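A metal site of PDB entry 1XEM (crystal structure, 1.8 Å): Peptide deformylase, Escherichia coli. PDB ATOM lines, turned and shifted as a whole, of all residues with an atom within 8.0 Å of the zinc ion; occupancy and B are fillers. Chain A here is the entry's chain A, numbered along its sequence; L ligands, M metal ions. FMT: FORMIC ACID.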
ATOM      1  N   VAL A   5      20.010   3.839  34.817  1.00  0.00           N
ATOM      2  CA  VAL A   5      20.307   4.833  33.783  1.00  0.00           C
ATOM      3  C   VAL A   5      20.244   4.193  32.401  1.00  0.00           C
ATOM      4  O   VAL A   5      20.944   3.192  32.127  1.00  0.00           O
ATOM      5  CB  VAL A   5      21.692   5.388  33.969  1.00  0.00           C
ATOM      6  CG1 VAL A   5      22.014   6.385  32.858  1.00  0.00           C
ATOM      7  CG2 VAL A   5      21.787   6.053  35.398  1.00  0.00           C
ATOM      8  N   LEU A  13      15.566   7.531  25.290  1.00  0.00           N
ATOM      9  CA  LEU A  13      16.447   8.690  25.458  1.00  0.00           C
ATOM     10  C   LEU A  13      16.154   9.840  24.452  1.00  0.00           C
ATOM     11  O   LEU A  13      16.728  10.931  24.585  1.00  0.00           O
ATOM     12  CB  LEU A  13      17.926   8.276  25.292  1.00  0.00           C
ATOM     13  CG  LEU A  13      18.398   7.380  26.411  1.00  0.00           C
ATOM     14  CD1 LEU A  13      19.811   6.761  26.030  1.00  0.00           C
ATOM     15  CD2 LEU A  13      18.629   8.268  27.654  1.00  0.00           C
ATOM     16  N   GLY A  45      26.249  15.444  36.178  1.00  0.00           N
ATOM     17  CA  GLY A  45      24.896  15.878  35.859  1.00  0.00           C
ATOM     18  C   GLY A  45      24.002  14.678  35.538  1.00  0.00           C
ATOM     19  O   GLY A  45      24.490  13.593  35.199  1.00  0.00           O
ATOM     20  N   LEU A  46      22.694  14.834  35.652  1.00  0.00           N
ATOM     21  CA  LEU A  46      21.806  13.769  35.226  1.00  0.00           C
ATOM     22  C   LEU A  46      20.437  14.417  34.875  1.00  0.00           C
ATOM     23  O   LEU A  46      19.928  15.290  35.612  1.00  0.00           O
ATOM     24  CB  LEU A  46      21.653  12.740  36.372  1.00  0.00           C
ATOM     25  CG  LEU A  46      20.722  11.538  36.120  1.00  0.00           C
ATOM     26  CD1 LEU A  46      21.395  10.609  34.956  1.00  0.00           C
ATOM     27  CD2 LEU A  46      20.641  10.699  37.367  1.00  0.00           C
ATOM     28  N   ALA A  47      19.865  14.005  33.746  1.00  0.00           N
ATOM     29  CA  ALA A  47      18.570  14.531  33.340  1.00  0.00           C
ATOM     30  C   ALA A  47      17.513  13.429  33.591  1.00  0.00           C
ATOM     31  O   ALA A  47      17.763  12.229  33.415  1.00  0.00           O
ATOM     32  CB  ALA A  47      18.606  14.923  31.887  1.00  0.00           C
ATOM     33  N   GLN A  50      17.078  10.459  31.232  1.00  0.00           N
ATOM     34  CA  GLN A  50      18.052   9.375  31.408  1.00  0.00           C
ATOM     35  C   GLN A  50      17.639   8.263  32.356  1.00  0.00           C
ATOM     36  O   GLN A  50      18.241   7.176  32.270  1.00  0.00           O
ATOM     37  CB  GLN A  50      19.376   9.927  31.893  1.00  0.00           C
ATOM     38  CG  GLN A  50      20.040  10.829  30.829  1.00  0.00           C
ATOM     39  CD  GLN A  50      21.355  11.289  31.340  1.00  0.00           C
ATOM     40  OE1 GLN A  50      21.438  12.349  32.021  1.00  0.00           O
ATOM     41  NE2 GLN A  50      22.417  10.508  31.028  1.00  0.00           N
ATOM     42  N   GLU A  88      33.336  15.849  26.406  1.00  0.00           N
ATOM     43  CA  GLU A  88      32.275  15.463  27.301  1.00  0.00           C
ATOM     44  C   GLU A  88      32.033  13.998  27.381  1.00  0.00           C
ATOM     45  O   GLU A  88      32.219  13.329  26.417  1.00  0.00           O
ATOM     46  CB  GLU A  88      30.950  16.105  26.818  1.00  0.00           C
ATOM     47  CG  GLU A  88      30.957  17.632  26.974  1.00  0.00           C
ATOM     48  CD  GLU A  88      29.691  18.302  26.470  1.00  0.00           C
ATOM     49  OE1 GLU A  88      28.617  17.677  26.625  1.00  0.00           O
ATOM     50  OE2 GLU A  88      29.745  19.424  25.914  1.00  0.00           O
ATOM     51  N   GLY A  89      31.596  13.538  28.543  1.00  0.00           N
ATOM     52  CA  GLY A  89      31.132  12.165  28.664  1.00  0.00           C
ATOM     53  C   GLY A  89      29.622  12.151  28.981  1.00  0.00           C
ATOM     54  O   GLY A  89      29.037  13.239  29.196  1.00  0.00           O
ATOM     55  N   CYS A  90      29.014  10.979  29.094  1.00  0.00           N
ATOM     56  CA  CYS A  90      27.593  10.909  29.410  1.00  0.00           C
ATOM     57  C   CYS A  90      27.317   9.538  29.994  1.00  0.00           C
ATOM     58  O   CYS A  90      27.758   8.510  29.413  1.00  0.00           O
ATOM     59  CB  CYS A  90      26.784  11.062  28.132  1.00  0.00           C
ATOM     60  SG  CYS A  90      24.977  10.992  28.362  1.00  0.00           S
ATOM     61  N   LEU A  91      26.605   9.499  31.108  1.00  0.00           N
ATOM     62  CA  LEU A  91      26.259   8.203  31.681  1.00  0.00           C
ATOM     63  C   LEU A  91      25.461   7.312  30.759  1.00  0.00           C
ATOM     64  O   LEU A  91      25.445   6.099  30.933  1.00  0.00           O
ATOM     65  CB  LEU A  91      25.497   8.377  32.994  1.00  0.00           C
ATOM     66  CG  LEU A  91      26.201   9.246  34.057  1.00  0.00           C
ATOM     67  CD1 LEU A  91      25.291   9.364  35.263  1.00  0.00           C
ATOM     68  CD2 LEU A  91      27.491   8.559  34.483  1.00  0.00           C
ATOM     69  N   SER A  92      24.776   7.883  29.782  1.00  0.00           N
ATOM     70  CA  SER A  92      23.961   7.083  28.859  1.00  0.00           C
ATOM     71  C   SER A  92      24.775   6.649  27.661  1.00  0.00           C
ATOM     72  O   SER A  92      24.244   5.948  26.799  1.00  0.00           O
ATOM     73  CB  SER A  92      22.736   7.870  28.376  1.00  0.00           C
ATOM     74  OG  SER A  92      21.808   8.068  29.427  1.00  0.00           O
ATOM     75  N   ILE A  93      26.035   7.077  27.567  1.00  0.00           N
ATOM     76  CA  ILE A  93      26.959   6.662  26.450  1.00  0.00           C
ATOM     77  C   ILE A  93      28.262   6.276  27.211  1.00  0.00           C
ATOM     78  O   ILE A  93      29.315   6.888  27.111  1.00  0.00           O
ATOM     79  CB  ILE A  93      27.200   7.804  25.509  1.00  0.00           C
ATOM     80  CG1 ILE A  93      25.864   8.421  25.128  1.00  0.00           C
ATOM     81  CG2 ILE A  93      27.946   7.307  24.248  1.00  0.00           C
ATOM     82  CD1 ILE A  93      26.048   9.648  24.184  1.00  0.00           C
ATOM     83  N   ARG A 102      29.819  24.227  22.378  1.00  0.00           N
ATOM     84  CA  ARG A 102      28.854  24.712  23.375  1.00  0.00           C
ATOM     85  C   ARG A 102      29.036  26.220  23.494  1.00  0.00           C
ATOM     86  O   ARG A 102      30.099  26.751  23.213  1.00  0.00           O
ATOM     87  CB  ARG A 102      29.198  24.119  24.788  1.00  0.00           C
ATOM     88  CG  ARG A 102      29.088  22.638  24.819  1.00  0.00           C
ATOM     89  CD  ARG A 102      27.605  22.242  24.766  1.00  0.00           C
ATOM     90  NE  ARG A 102      27.469  20.807  25.103  1.00  0.00           N
ATOM     91  CZ  ARG A 102      26.376  20.054  24.894  1.00  0.00           C
ATOM     92  NH1 ARG A 102      25.272  20.564  24.377  1.00  0.00           N
ATOM     93  NH2 ARG A 102      26.381  18.755  25.140  1.00  0.00           N
ATOM     94  N   CYS A 129      27.883  21.782  31.306  1.00  0.00           N
ATOM     95  CA  CYS A 129      27.089  20.735  31.875  1.00  0.00           C
ATOM     96  C   CYS A 129      25.611  21.126  31.753  1.00  0.00           C
ATOM     97  O   CYS A 129      24.750  20.263  31.459  1.00  0.00           O
ATOM     98  CB  CYS A 129      27.518  20.514  33.358  1.00  0.00           C
ATOM     99  SG  CYS A 129      26.613  19.235  34.240  1.00  0.00           S
ATOM    100  N   HIS A 132      24.498  20.423  28.228  1.00  0.00           N
ATOM    101  CA  HIS A 132      24.406  18.977  27.992  1.00  0.00           C
ATOM    102  C   HIS A 132      23.138  18.418  28.621  1.00  0.00           C
ATOM    103  O   HIS A 132      22.434  17.626  27.982  1.00  0.00           O
ATOM    104  CB  HIS A 132      25.635  18.341  28.649  1.00  0.00           C
ATOM    105  CG  HIS A 132      25.701  16.854  28.593  1.00  0.00           C
ATOM    106  ND1 HIS A 132      26.677  16.191  27.888  1.00  0.00           N
ATOM    107  CD2 HIS A 132      24.923  15.907  29.166  1.00  0.00           C
ATOM    108  CE1 HIS A 132      26.485  14.871  28.029  1.00  0.00           C
ATOM    109  NE2 HIS A 132      25.447  14.641  28.797  1.00  0.00           N
ATOM    110  N   GLU A 133      22.833  18.808  29.866  1.00  0.00           N
ATOM    111  CA  GLU A 133      21.658  18.243  30.505  1.00  0.00           C
ATOM    112  C   GLU A 133      20.351  18.781  29.888  1.00  0.00           C
ATOM    113  O   GLU A 133      19.345  18.036  29.806  1.00  0.00           O
ATOM    114  CB  GLU A 133      21.662  18.476  32.045  1.00  0.00           C
ATOM    115  CG  GLU A 133      22.939  17.883  32.777  1.00  0.00           C
ATOM    116  CD  GLU A 133      23.192  16.459  32.472  1.00  0.00           C
ATOM    117  OE1 GLU A 133      22.237  15.742  32.187  1.00  0.00           O
ATOM    118  OE2 GLU A 133      24.380  16.033  32.487  1.00  0.00           O
ATOM    119  N   ASP A 135      19.967  19.479  26.875  1.00  0.00           N
ATOM    120  CA  ASP A 135      19.763  18.761  25.618  1.00  0.00           C
ATOM    121  C   ASP A 135      19.052  17.425  25.874  1.00  0.00           C
ATOM    122  O   ASP A 135      18.241  17.010  25.069  1.00  0.00           O
ATOM    123  CB  ASP A 135      21.092  18.444  24.957  1.00  0.00           C
ATOM    124  CG  ASP A 135      21.646  19.573  24.095  1.00  0.00           C
ATOM    125  OD1 ASP A 135      21.014  20.627  23.898  1.00  0.00           O
ATOM    126  OD2 ASP A 135      22.763  19.393  23.558  1.00  0.00           O
ATOM    127  N   HIS A 136      19.406  16.739  26.961  1.00  0.00           N
ATOM    128  CA  HIS A 136      18.758  15.469  27.250  1.00  0.00           C
ATOM    129  C   HIS A 136      17.229  15.592  27.294  1.00  0.00           C
ATOM    130  O   HIS A 136      16.532  14.669  26.819  1.00  0.00           O
ATOM    131  CB  HIS A 136      19.212  14.882  28.600  1.00  0.00           C
ATOM    132  CG  HIS A 136      20.471  14.096  28.504  1.00  0.00           C
ATOM    133  ND1 HIS A 136      20.626  12.988  27.699  1.00  0.00           N
ATOM    134  CD2 HIS A 136      21.648  14.245  29.165  1.00  0.00           C
ATOM    135  CE1 HIS A 136      21.880  12.487  27.900  1.00  0.00           C
ATOM    136  NE2 HIS A 136      22.538  13.208  28.778  1.00  0.00           N
ATOM    137  N   LYS A 140      18.117  14.992  22.939  1.00  0.00           N
ATOM    138  CA  LYS A 140      19.354  15.228  22.192  1.00  0.00           C
ATOM    139  C   LYS A 140      20.544  14.735  23.020  1.00  0.00           C
ATOM    140  O   LYS A 140      20.629  14.960  24.266  1.00  0.00           O
ATOM    141  CB  LYS A 140      19.503  16.713  21.856  1.00  0.00           C
ATOM    142  CG  LYS A 140      20.732  17.034  21.045  1.00  0.00           C
ATOM    143  CD  LYS A 140      20.599  18.496  20.540  1.00  0.00           C
ATOM    144  CE  LYS A 140      21.715  18.767  19.493  1.00  0.00           C
ATOM    145  NZ  LYS A 140      21.640  20.261  19.060  1.00  0.00           N
ATOM    146  N   LEU A 141      21.472  14.064  22.334  1.00  0.00           N
ATOM    147  CA  LEU A 141      22.664  13.469  23.002  1.00  0.00           C
ATOM    148  C   LEU A 141      23.912  14.118  22.404  1.00  0.00           C
ATOM    149  O   LEU A 141      23.865  14.676  21.297  1.00  0.00           O
ATOM    150  CB  LEU A 141      22.745  11.952  22.777  1.00  0.00           C
ATOM    151  CG  LEU A 141      21.523  11.164  23.145  1.00  0.00           C
ATOM    152  CD1 LEU A 141      21.797   9.674  22.760  1.00  0.00           C
ATOM    153  CD2 LEU A 141      21.302  11.265  24.618  1.00  0.00           C
ATOM    154  N   PHE A 142      25.005  14.098  23.142  1.00  0.00           N
ATOM    155  CA  PHE A 142      26.154  14.865  22.675  1.00  0.00           C
ATOM    156  C   PHE A 142      26.703  14.303  21.368  1.00  0.00           C
ATOM    157  O   PHE A 142      27.304  15.016  20.539  1.00  0.00           O
ATOM    158  CB  PHE A 142      27.239  14.975  23.792  1.00  0.00           C
ATOM    159  CG  PHE A 142      28.124  13.738  23.924  1.00  0.00           C
ATOM    160  CD1 PHE A 142      29.124  13.467  22.996  1.00  0.00           C
ATOM    161  CD2 PHE A 142      28.001  12.900  25.016  1.00  0.00           C
ATOM    162  CE1 PHE A 142      29.919  12.327  23.112  1.00  0.00           C
ATOM    163  CE2 PHE A 142      28.806  11.749  25.140  1.00  0.00           C
ATOM    164  CZ  PHE A 142      29.787  11.500  24.207  1.00  0.00           C
HETATM  165  C   FMT L   1      25.232  12.978  31.968  1.00  0.00           C
HETATM  166  O1  FMT L   1      24.159  13.624  31.321  1.00  0.00           O
HETATM  167  O2  FMT L   1      24.980  11.566  31.839  1.00  0.00           O
HETATM  168 ZN    ZN M   1      24.415  12.927  29.369  1.00  0.00          ZN
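The side-chain sulfur (SG) of Cys 90 lies close to the side-chain amide nitrogen (NE2) of Gln 50 (3.7 Å).
A ring nitrogen (ND1) of His 132 is in hydrogen-bond range of the side-chain carboxylate (OE1) of Glu 88, at 2.8 Å.
The side-chain amide oxygen (OE1) of Gln 50 sits at hydrogen-bond distance from the backbone NH (N) of Ala 47, 2.9 Å away.
OE1 of Gln 50 sits close to OE1 of Glu 133 (3.5 Å).
The side-chain sulfur (SG) of Cys 90 lies close to the backbone NH (N) of Ser 92, at 3.4 Å.
The side-chain hydroxyl (OG) of Ser 92 sits at hydrogen-bond distance from the side-chain amide nitrogen (NE2) of Gln 50, at 3.0 Å.
Merely in contact with the zinc ion: Gln 50.
Of the 21 residues printed, 4 come within 4 Å of the zinc ion.
The nearest printed residue that does not touch the zinc ion is Glu 133 (4.4 Å).
The zinc ion is bound by a ring nitrogen (NE2) of His 136, a ring nitrogen (NE2) of His 132, an oxygen (O1) of the ligand and the side-chain sulfur (SG) of Cys 90.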
